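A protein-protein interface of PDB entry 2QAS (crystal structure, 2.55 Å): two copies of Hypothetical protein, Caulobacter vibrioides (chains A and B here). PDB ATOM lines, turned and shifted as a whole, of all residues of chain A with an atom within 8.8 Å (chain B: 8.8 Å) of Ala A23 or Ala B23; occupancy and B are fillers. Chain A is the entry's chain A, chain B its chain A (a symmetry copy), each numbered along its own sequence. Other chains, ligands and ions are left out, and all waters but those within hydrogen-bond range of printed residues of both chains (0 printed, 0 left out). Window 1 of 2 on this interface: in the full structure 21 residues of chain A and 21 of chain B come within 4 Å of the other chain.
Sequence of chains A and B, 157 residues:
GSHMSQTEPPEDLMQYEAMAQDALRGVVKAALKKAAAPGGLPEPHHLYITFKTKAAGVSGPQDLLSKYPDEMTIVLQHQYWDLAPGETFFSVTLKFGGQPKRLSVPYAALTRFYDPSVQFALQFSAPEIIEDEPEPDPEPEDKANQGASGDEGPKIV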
ATOM      1  N   TYR A  16      10.038   3.687  -9.589  1.00  0.00           N
ATOM      2  CA  TYR A  16       9.781   2.331  -9.156  1.00  0.00           C
ATOM      3  C   TYR A  16      10.837   1.384  -9.693  1.00  0.00           C
ATOM      4  O   TYR A  16      11.325   0.512  -8.972  1.00  0.00           O
ATOM      5  CB  TYR A  16       8.386   1.880  -9.603  1.00  0.00           C
ATOM      6  CG  TYR A  16       7.274   2.474  -8.770  1.00  0.00           C
ATOM      7  CD1 TYR A  16       6.279   3.264  -9.350  1.00  0.00           C
ATOM      8  CD2 TYR A  16       7.213   2.242  -7.393  1.00  0.00           C
ATOM      9  CE1 TYR A  16       5.247   3.807  -8.576  1.00  0.00           C
ATOM     10  CE2 TYR A  16       6.186   2.779  -6.611  1.00  0.00           C
ATOM     11  CZ  TYR A  16       5.207   3.559  -7.211  1.00  0.00           C
ATOM     12  OH  TYR A  16       4.194   4.089  -6.446  1.00  0.00           O
ATOM     13  N   GLU A  17      11.200   1.570 -10.957  1.00  0.00           N
ATOM     14  CA  GLU A  17      12.194   0.705 -11.574  1.00  0.00           C
ATOM     15  C   GLU A  17      13.554   0.770 -10.879  1.00  0.00           C
ATOM     16  O   GLU A  17      14.238  -0.243 -10.740  1.00  0.00           O
ATOM     17  CB  GLU A  17      12.344   1.036 -13.062  1.00  0.00           C
ATOM     18  CG  GLU A  17      12.910  -0.137 -13.831  1.00  0.00           C
ATOM     19  CD  GLU A  17      12.361  -1.465 -13.301  1.00  0.00           C
ATOM     20  OE1 GLU A  17      11.112  -1.633 -13.275  1.00  0.00           O
ATOM     21  OE2 GLU A  17      13.181  -2.330 -12.897  1.00  0.00           O
ATOM     22  N   ALA A  18      13.938   1.962 -10.437  1.00  0.00           N
ATOM     23  CA  ALA A  18      15.200   2.127  -9.738  1.00  0.00           C
ATOM     24  C   ALA A  18      15.116   1.452  -8.372  1.00  0.00           C
ATOM     25  O   ALA A  18      16.052   0.779  -7.957  1.00  0.00           O
ATOM     26  CB  ALA A  18      15.520   3.599  -9.571  1.00  0.00           C
ATOM     27  N   MET A  19      13.992   1.626  -7.680  1.00  0.00           N
ATOM     28  CA  MET A  19      13.814   1.019  -6.358  1.00  0.00           C
ATOM     29  C   MET A  19      13.793  -0.504  -6.447  1.00  0.00           C
ATOM     30  O   MET A  19      14.212  -1.194  -5.521  1.00  0.00           O
ATOM     31  CB  MET A  19      12.510   1.495  -5.712  1.00  0.00           C
ATOM     32  CG  MET A  19      12.437   2.977  -5.394  1.00  0.00           C
ATOM     33  SD  MET A  19      10.782   3.389  -4.788  1.00  0.00           S
ATOM     34  CE  MET A  19      11.152   3.976  -3.188  1.00  0.00           C
ATOM     35  N   ALA A  20      13.289  -1.029  -7.555  1.00  0.00           N
ATOM     36  CA  ALA A  20      13.242  -2.472  -7.746  1.00  0.00           C
ATOM     37  C   ALA A  20      14.659  -3.007  -7.978  1.00  0.00           C
ATOM     38  O   ALA A  20      14.975  -4.136  -7.603  1.00  0.00           O
ATOM     39  CB  ALA A  20      12.349  -2.814  -8.934  1.00  0.00           C
ATOM     40  N   GLN A  21      15.498  -2.182  -8.597  1.00  0.00           N
ATOM     41  CA  GLN A  21      16.882  -2.538  -8.892  1.00  0.00           C
ATOM     42  C   GLN A  21      17.673  -2.654  -7.587  1.00  0.00           C
ATOM     43  O   GLN A  21      18.388  -3.624  -7.373  1.00  0.00           O
ATOM     44  CB  GLN A  21      17.514  -1.465  -9.781  1.00  0.00           C
ATOM     45  CG  GLN A  21      18.536  -1.982 -10.781  1.00  0.00           C
ATOM     46  CD  GLN A  21      17.885  -2.680 -11.968  1.00  0.00           C
ATOM     47  OE1 GLN A  21      17.122  -3.641 -11.805  1.00  0.00           O
ATOM     48  NE2 GLN A  21      18.192  -2.201 -13.175  1.00  0.00           N
ATOM     49  N   ASP A  22      17.543  -1.657  -6.719  1.00  0.00           N
ATOM     50  CA  ASP A  22      18.235  -1.672  -5.437  1.00  0.00           C
ATOM     51  C   ASP A  22      17.745  -2.837  -4.608  1.00  0.00           C
ATOM     52  O   ASP A  22      18.535  -3.566  -4.011  1.00  0.00           O
ATOM     53  CB  ASP A  22      17.974  -0.387  -4.662  1.00  0.00           C
ATOM     54  CG  ASP A  22      18.410   0.834  -5.417  1.00  0.00           C
ATOM     55  OD1 ASP A  22      19.567   0.843  -5.901  1.00  0.00           O
ATOM     56  OD2 ASP A  22      17.600   1.783  -5.530  1.00  0.00           O
ATOM     57  N   ALA A  23      16.429  -2.993  -4.557  1.00  0.00           N
ATOM     58  CA  ALA A  23      15.837  -4.077  -3.802  1.00  0.00           C
ATOM     59  C   ALA A  23      16.491  -5.390  -4.214  1.00  0.00           C
ATOM     60  O   ALA A  23      16.825  -6.216  -3.371  1.00  0.00           O
ATOM     61  CB  ALA A  23      14.329  -4.137  -4.059  1.00  0.00           C
ATOM     62  N   LEU A  24      16.691  -5.571  -5.513  1.00  0.00           N
ATOM     63  CA  LEU A  24      17.274  -6.803  -6.008  1.00  0.00           C
ATOM     64  C   LEU A  24      18.772  -6.985  -5.734  1.00  0.00           C
ATOM     65  O   LEU A  24      19.263  -8.117  -5.699  1.00  0.00           O
ATOM     66  CB  LEU A  24      16.969  -6.953  -7.498  1.00  0.00           C
ATOM     67  CG  LEU A  24      15.492  -7.269  -7.737  1.00  0.00           C
ATOM     68  CD1 LEU A  24      15.195  -7.297  -9.224  1.00  0.00           C
ATOM     69  CD2 LEU A  24      15.154  -8.610  -7.091  1.00  0.00           C
ATOM     70  N   ARG A  25      19.501  -5.890  -5.540  1.00  0.00           N
ATOM     71  CA  ARG A  25      20.920  -6.013  -5.228  1.00  0.00           C
ATOM     72  C   ARG A  25      21.008  -6.775  -3.913  1.00  0.00           C
ATOM     73  O   ARG A  25      21.994  -7.470  -3.643  1.00  0.00           O
ATOM     74  CB  ARG A  25      21.574  -4.636  -5.080  1.00  0.00           C
ATOM     75  CG  ARG A  25      21.728  -3.883  -6.398  1.00  0.00           C
ATOM     76  CD  ARG A  25      22.443  -2.555  -6.200  1.00  0.00           C
ATOM     77  NE  ARG A  25      22.622  -1.840  -7.465  1.00  0.00           N
ATOM     78  CZ  ARG A  25      23.446  -2.225  -8.437  1.00  0.00           C
ATOM     79  NH1 ARG A  25      24.177  -3.324  -8.295  1.00  0.00           N
ATOM     80  NH2 ARG A  25      23.538  -1.513  -9.556  1.00  0.00           N
ATOM     81  N   GLY A  26      19.951  -6.653  -3.114  1.00  0.00           N
ATOM     82  CA  GLY A  26      19.887  -7.321  -1.828  1.00  0.00           C
ATOM     83  C   GLY A  26      19.894  -8.835  -1.911  1.00  0.00           C
ATOM     84  O   GLY A  26      20.196  -9.505  -0.921  1.00  0.00           O
ATOM     85  N   VAL A  27      19.548  -9.384  -3.072  1.00  0.00           N
ATOM     86  CA  VAL A  27      19.553 -10.838  -3.243  1.00  0.00           C
ATOM     87  C   VAL A  27      21.011 -11.300  -3.301  1.00  0.00           C
ATOM     88  O   VAL A  27      21.360 -12.379  -2.818  1.00  0.00           O
ATOM     89  CB  VAL A  27      18.835 -11.273  -4.544  1.00  0.00           C
ATOM     90  CG1 VAL A  27      19.019 -12.769  -4.769  1.00  0.00           C
ATOM     91  CG2 VAL A  27      17.357 -10.953  -4.454  1.00  0.00           C
ATOM     92  N   VAL A  28      21.859 -10.469  -3.896  1.00  0.00           N
ATOM     93  CA  VAL A  28      23.276 -10.788  -3.993  1.00  0.00           C
ATOM     94  C   VAL A  28      23.840 -10.846  -2.583  1.00  0.00           C
ATOM     95  O   VAL A  28      24.538 -11.787  -2.214  1.00  0.00           O
ATOM     96  CB  VAL A  28      24.025  -9.719  -4.802  1.00  0.00           C
ATOM     97  CG1 VAL A  28      25.509 -10.024  -4.818  1.00  0.00           C
ATOM     98  CG2 VAL A  28      23.461  -9.669  -6.232  1.00  0.00           C
ATOM     99  N   LYS A  29      23.521  -9.837  -1.787  1.00  0.00           N
ATOM    100  CA  LYS A  29      23.988  -9.786  -0.411  1.00  0.00           C
ATOM    101  C   LYS A  29      23.511 -10.980   0.397  1.00  0.00           C
ATOM    102  O   LYS A  29      24.258 -11.544   1.198  1.00  0.00           O
ATOM    103  CB  LYS A  29      23.496  -8.509   0.239  1.00  0.00           C
ATOM    104  CG  LYS A  29      23.648  -8.473   1.730  1.00  0.00           C
ATOM    105  CD  LYS A  29      23.231  -7.106   2.201  1.00  0.00           C
ATOM    106  CE  LYS A  29      23.182  -7.015   3.703  1.00  0.00           C
ATOM    107  NZ  LYS A  29      22.553  -5.719   4.069  1.00  0.00           N
ATOM    108  N   ALA A  30      22.263 -11.374   0.195  1.00  0.00           N
ATOM    109  CA  ALA A  30      21.738 -12.511   0.936  1.00  0.00           C
ATOM    110  C   ALA A  30      22.389 -13.813   0.471  1.00  0.00           C
ATOM    111  O   ALA A  30      22.618 -14.713   1.276  1.00  0.00           O
ATOM    112  CB  ALA A  30      20.234 -12.584   0.787  1.00  0.00           C
ATOM    113  N   LEU A 122      20.763 -11.990 -12.702  1.00  0.00           N
ATOM    114  CA  LEU A 122      20.273 -10.647 -12.386  1.00  0.00           C
ATOM    115  C   LEU A 122      21.181  -9.634 -13.069  1.00  0.00           C
ATOM    116  O   LEU A 122      22.377  -9.869 -13.196  1.00  0.00           O
ATOM    117  CB  LEU A 122      20.301 -10.389 -10.874  1.00  0.00           C
ATOM    118  CG  LEU A 122      19.360 -11.179  -9.965  1.00  0.00           C
ATOM    119  CD1 LEU A 122      19.652 -10.822  -8.514  1.00  0.00           C
ATOM    120  CD2 LEU A 122      17.908 -10.865 -10.306  1.00  0.00           C
ATOM    121  N   PHE A 124      22.035  -5.390 -13.048  1.00  0.00           N
ATOM    122  CA  PHE A 124      21.796  -4.102 -12.399  1.00  0.00           C
ATOM    123  C   PHE A 124      22.437  -2.932 -13.133  1.00  0.00           C
ATOM    124  O   PHE A 124      22.934  -3.071 -14.251  1.00  0.00           O
ATOM    125  CB  PHE A 124      22.332  -4.096 -10.964  1.00  0.00           C
ATOM    126  CG  PHE A 124      22.072  -5.358 -10.203  1.00  0.00           C
ATOM    127  CD1 PHE A 124      22.936  -6.436 -10.309  1.00  0.00           C
ATOM    128  CD2 PHE A 124      20.976  -5.461  -9.364  1.00  0.00           C
ATOM    129  CE1 PHE A 124      22.713  -7.598  -9.589  1.00  0.00           C
ATOM    130  CE2 PHE A 124      20.745  -6.619  -8.641  1.00  0.00           C
ATOM    131  CZ  PHE A 124      21.616  -7.690  -8.753  1.00  0.00           C
ATOM    132  N   TYR B  16      16.352 -18.717  -4.699  1.00  0.00           N
ATOM    133  CA  TYR B  16      16.553 -17.409  -5.285  1.00  0.00           C
ATOM    134  C   TYR B  16      15.229 -16.701  -5.492  1.00  0.00           C
ATOM    135  O   TYR B  16      15.103 -15.508  -5.210  1.00  0.00           O
ATOM    136  CB  TYR B  16      17.306 -17.528  -6.615  1.00  0.00           C
ATOM    137  CG  TYR B  16      18.783 -17.799  -6.440  1.00  0.00           C
ATOM    138  CD1 TYR B  16      19.375 -18.946  -6.975  1.00  0.00           C
ATOM    139  CD2 TYR B  16      19.594 -16.902  -5.741  1.00  0.00           C
ATOM    140  CE1 TYR B  16      20.744 -19.190  -6.816  1.00  0.00           C
ATOM    141  CE2 TYR B  16      20.963 -17.137  -5.578  1.00  0.00           C
ATOM    142  CZ  TYR B  16      21.529 -18.283  -6.120  1.00  0.00           C
ATOM    143  OH  TYR B  16      22.876 -18.518  -5.964  1.00  0.00           O
ATOM    144  N   GLU B  17      14.236 -17.444  -5.968  1.00  0.00           N
ATOM    145  CA  GLU B  17      12.929 -16.857  -6.218  1.00  0.00           C
ATOM    146  C   GLU B  17      12.278 -16.295  -4.954  1.00  0.00           C
ATOM    147  O   GLU B  17      11.629 -15.249  -4.993  1.00  0.00           O
ATOM    148  CB  GLU B  17      12.001 -17.877  -6.883  1.00  0.00           C
ATOM    149  CG  GLU B  17      10.883 -17.192  -7.639  1.00  0.00           C
ATOM    150  CD  GLU B  17      11.378 -15.912  -8.321  1.00  0.00           C
ATOM    151  OE1 GLU B  17      12.345 -15.993  -9.124  1.00  0.00           O
ATOM    152  OE2 GLU B  17      10.806 -14.828  -8.038  1.00  0.00           O
ATOM    153  N   ALA B  18      12.457 -16.987  -3.836  1.00  0.00           N
ATOM    154  CA  ALA B  18      11.904 -16.525  -2.576  1.00  0.00           C
ATOM    155  C   ALA B  18      12.644 -15.269  -2.126  1.00  0.00           C
ATOM    156  O   ALA B  18      12.024 -14.316  -1.668  1.00  0.00           O
ATOM    157  CB  ALA B  18      12.025 -17.605  -1.520  1.00  0.00           C
ATOM    158  N   MET B  19      13.968 -15.265  -2.264  1.00  0.00           N
ATOM    159  CA  MET B  19      14.770 -14.107  -1.862  1.00  0.00           C
ATOM    160  C   MET B  19      14.448 -12.886  -2.720  1.00  0.00           C
ATOM    161  O   MET B  19      14.531 -11.752  -2.256  1.00  0.00           O
ATOM    162  CB  MET B  19      16.265 -14.412  -1.977  1.00  0.00           C
ATOM    163  CG  MET B  19      16.787 -15.497  -1.054  1.00  0.00           C
ATOM    164  SD  MET B  19      18.524 -15.837  -1.433  1.00  0.00           S
ATOM    165  CE  MET B  19      19.281 -15.426   0.084  1.00  0.00           C
ATOM    166  N   ALA B  20      14.097 -13.119  -3.977  1.00  0.00           N
ATOM    167  CA  ALA B  20      13.751 -12.024  -4.872  1.00  0.00           C
ATOM    168  C   ALA B  20      12.399 -11.431  -4.464  1.00  0.00           C
ATOM    169  O   ALA B  20      12.157 -10.237  -4.631  1.00  0.00           O
ATOM    170  CB  ALA B  20      13.694 -12.523  -6.312  1.00  0.00           C
ATOM    171  N   GLN B  21      11.529 -12.284  -3.928  1.00  0.00           N
ATOM    172  CA  GLN B  21      10.199 -11.880  -3.485  1.00  0.00           C
ATOM    173  C   GLN B  21      10.319 -10.958  -2.270  1.00  0.00           C
ATOM    174  O   GLN B  21       9.699  -9.904  -2.221  1.00  0.00           O
ATOM    175  CB  GLN B  21       9.381 -13.118  -3.111  1.00  0.00           C
ATOM    176  CG  GLN B  21       7.893 -13.014  -3.401  1.00  0.00           C
ATOM    177  CD  GLN B  21       7.578 -13.170  -4.883  1.00  0.00           C
ATOM    178  OE1 GLN B  21       8.095 -12.428  -5.728  1.00  0.00           O
ATOM    179  NE2 GLN B  21       6.718 -14.139  -5.205  1.00  0.00           N
ATOM    180  N   ASP B  22      11.118 -11.363  -1.289  1.00  0.00           N
ATOM    181  CA  ASP B  22      11.321 -10.555  -0.094  1.00  0.00           C
ATOM    182  C   ASP B  22      11.974  -9.245  -0.471  1.00  0.00           C
ATOM    183  O   ASP B  22      11.565  -8.179  -0.014  1.00  0.00           O
ATOM    184  CB  ASP B  22      12.223 -11.273   0.902  1.00  0.00           C
ATOM    185  CG  ASP B  22      11.665 -12.601   1.323  1.00  0.00           C
ATOM    186  OD1 ASP B  22      10.471 -12.642   1.704  1.00  0.00           O
ATOM    187  OD2 ASP B  22      12.416 -13.603   1.270  1.00  0.00           O
ATOM    188  N   ALA B  23      13.012  -9.335  -1.291  1.00  0.00           N
ATOM    189  CA  ALA B  23      13.718  -8.150  -1.732  1.00  0.00           C
ATOM    190  C   ALA B  23      12.714  -7.147  -2.286  1.00  0.00           C
ATOM    191  O   ALA B  23      12.791  -5.958  -1.995  1.00  0.00           O
ATOM    192  CB  ALA B  23      14.744  -8.517  -2.807  1.00  0.00           C
ATOM    193  N   LEU B  24      11.761  -7.633  -3.071  1.00  0.00           N
ATOM    194  CA  LEU B  24      10.780  -6.753  -3.676  1.00  0.00           C
ATOM    195  C   LEU B  24       9.726  -6.178  -2.722  1.00  0.00           C
ATOM    196  O   LEU B  24       9.147  -5.124  -3.000  1.00  0.00           O
ATOM    197  CB  LEU B  24      10.119  -7.458  -4.859  1.00  0.00           C
ATOM    198  CG  LEU B  24      11.083  -7.597  -6.038  1.00  0.00           C
ATOM    199  CD1 LEU B  24      10.440  -8.401  -7.151  1.00  0.00           C
ATOM    200  CD2 LEU B  24      11.477  -6.206  -6.531  1.00  0.00           C
ATOM    201  N   ARG B  25       9.471  -6.853  -1.605  1.00  0.00           N
ATOM    202  CA  ARG B  25       8.513  -6.323  -0.643  1.00  0.00           C
ATOM    203  C   ARG B  25       9.071  -4.988  -0.169  1.00  0.00           C
ATOM    204  O   ARG B  25       8.323  -4.084   0.215  1.00  0.00           O
ATOM    205  CB  ARG B  25       8.343  -7.271   0.547  1.00  0.00           C
ATOM    206  CG  ARG B  25       7.590  -8.554   0.209  1.00  0.00           C
ATOM    207  CD  ARG B  25       7.392  -9.424   1.441  1.00  0.00           C
ATOM    208  NE  ARG B  25       6.643 -10.644   1.130  1.00  0.00           N
ATOM    209  CZ  ARG B  25       5.352 -10.673   0.809  1.00  0.00           C
ATOM    210  NH1 ARG B  25       4.653  -9.546   0.756  1.00  0.00           N
ATOM    211  NH2 ARG B  25       4.757 -11.830   0.536  1.00  0.00           N
ATOM    212  N   GLY B  26      10.396  -4.873  -0.229  1.00  0.00           N
ATOM    213  CA  GLY B  26      11.075  -3.661   0.187  1.00  0.00           C
ATOM    214  C   GLY B  26      10.737  -2.440  -0.647  1.00  0.00           C
ATOM    215  O   GLY B  26      10.953  -1.311  -0.203  1.00  0.00           O
ATOM    216  N   VAL B  27      10.226  -2.651  -1.857  1.00  0.00           N
ATOM    217  CA  VAL B  27       9.848  -1.526  -2.715  1.00  0.00           C
ATOM    218  C   VAL B  27       8.579  -0.897  -2.136  1.00  0.00           C
ATOM    219  O   VAL B  27       8.384   0.319  -2.191  1.00  0.00           O
ATOM    220  CB  VAL B  27       9.570  -1.974  -4.171  1.00  0.00           C
ATOM    221  CG1 VAL B  27       9.012  -0.808  -4.980  1.00  0.00           C
ATOM    222  CG2 VAL B  27      10.847  -2.471  -4.816  1.00  0.00           C
ATOM    223  N   VAL B  28       7.717  -1.739  -1.578  1.00  0.00           N
ATOM    224  CA  VAL B  28       6.484  -1.258  -0.973  1.00  0.00           C
ATOM    225  C   VAL B  28       6.856  -0.371   0.205  1.00  0.00           C
ATOM    226  O   VAL B  28       6.345   0.736   0.355  1.00  0.00           O
ATOM    227  CB  VAL B  28       5.620  -2.429  -0.482  1.00  0.00           C
ATOM    228  CG1 VAL B  28       4.384  -1.904   0.220  1.00  0.00           C
ATOM    229  CG2 VAL B  28       5.236  -3.319  -1.675  1.00  0.00           C
ATOM    230  N   LYS B  29       7.763  -0.860   1.037  1.00  0.00           N
ATOM    231  CA  LYS B  29       8.211  -0.100   2.192  1.00  0.00           C
ATOM    232  C   LYS B  29       8.837   1.226   1.795  1.00  0.00           C
ATOM    233  O   LYS B  29       8.612   2.252   2.438  1.00  0.00           O
ATOM    234  CB  LYS B  29       9.220  -0.919   2.971  1.00  0.00           C
ATOM    235  CG  LYS B  29       9.982  -0.147   4.006  1.00  0.00           C
ATOM    236  CD  LYS B  29      10.842  -1.121   4.764  1.00  0.00           C
ATOM    237  CE  LYS B  29      11.779  -0.426   5.716  1.00  0.00           C
ATOM    238  NZ  LYS B  29      12.733  -1.434   6.248  1.00  0.00           N
ATOM    239  N   ALA B  30       9.628   1.215   0.734  1.00  0.00           N
ATOM    240  CA  ALA B  30      10.263   2.449   0.295  1.00  0.00           C
ATOM    241  C   ALA B  30       9.233   3.416  -0.288  1.00  0.00           C
ATOM    242  O   ALA B  30       9.355   4.627  -0.120  1.00  0.00           O
ATOM    243  CB  ALA B  30      11.347   2.150  -0.717  1.00  0.00           C
ATOM    244  N   LEU B 122       3.132  -5.248  -8.486  1.00  0.00           N
ATOM    245  CA  LEU B 122       3.955  -6.296  -7.879  1.00  0.00           C
ATOM    246  C   LEU B 122       3.030  -7.324  -7.245  1.00  0.00           C
ATOM    247  O   LEU B 122       1.969  -6.971  -6.745  1.00  0.00           O
ATOM    248  CB  LEU B 122       4.868  -5.722  -6.789  1.00  0.00           C
ATOM    249  CG  LEU B 122       5.996  -4.767  -7.185  1.00  0.00           C
ATOM    250  CD1 LEU B 122       6.682  -4.257  -5.927  1.00  0.00           C
ATOM    251  CD2 LEU B 122       6.998  -5.479  -8.086  1.00  0.00           C
ATOM    252  N   PHE B 124       3.165 -10.693  -4.528  1.00  0.00           N
ATOM    253  CA  PHE B 124       3.976 -11.474  -3.596  1.00  0.00           C
ATOM    254  C   PHE B 124       3.261 -12.711  -3.069  1.00  0.00           C
ATOM    255  O   PHE B 124       2.187 -13.081  -3.545  1.00  0.00           O
ATOM    256  CB  PHE B 124       4.396 -10.634  -2.387  1.00  0.00           C
ATOM    257  CG  PHE B 124       4.811  -9.236  -2.721  1.00  0.00           C
ATOM    258  CD1 PHE B 124       3.866  -8.229  -2.840  1.00  0.00           C
ATOM    259  CD2 PHE B 124       6.147  -8.919  -2.896  1.00  0.00           C
ATOM    260  CE1 PHE B 124       4.245  -6.929  -3.126  1.00  0.00           C
ATOM    261  CE2 PHE B 124       6.536  -7.622  -3.183  1.00  0.00           C
ATOM    262  CZ  PHE B 124       5.582  -6.624  -3.298  1.00  0.00           C
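Among the printed residues, pairs that only touch across the chains: Met A19 with Val B27 (3.7 Å), Met A19 with Ala B30 (3.1 Å), Ala A20 with Val B27 (3.8 Å), Ala A23 with Ala B23 (3.2 Å), Ala A23 with Val B27 (3.9 Å), Val A27 with Met B19 (3.7 Å), Val A27 with Ala B20 (3.8 Å), Val A27 with Ala B23 (3.9 Å) and Ala A30 with Met B19 (3.1 Å).
Met A19 touches Ala B30, and with the chains exchanged Ala A30 touches Met B19.
Ala A20 touches Val B27, and with the chains exchanged Val A27 touches Ala B20.
Ala A23 touches its own counterpart, Ala B23.
Ala A23 touches Val B27, and with the chains exchanged Val A27 touches Ala B23.
Of the 9 pairs that touch across the chains among the printed residues, 9 have their exchanged pair printed and touching as well.
Of the 17 printed residues of chain B, 5 touch a printed residue of chain A.
Of the 17 printed residues of chain A, 5 touch a printed residue of chain B.
Printed residues of chain A that touch a printed residue of chain B: Met A19, Ala A20, Ala A23, Val A27 and Ala A30.
Hydrophobic or aromatic side chains of chain A within 4 Å of the printed part of chain B: Met A19, Ala A23, Val A27 and Ala A30.
Among the printed residues, no Asp or Glu carboxylate lies within 4 Å of a Lys or Arg side-chain nitrogen of the other chain.
Ala A23 touches two residues of chain B.
Of chain A, only Ala A23 and Val A27 come within 4 Å of Ala B23.
Of the printed residues of chain B, Ala A20 touches Val B27.
Printed residues of chain B within 4 Å of Ala A30: Met B19 (3.1 Å).
The nearest residue of chain B that does not touch Ala A23 is Leu B24 (4.3 Å).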
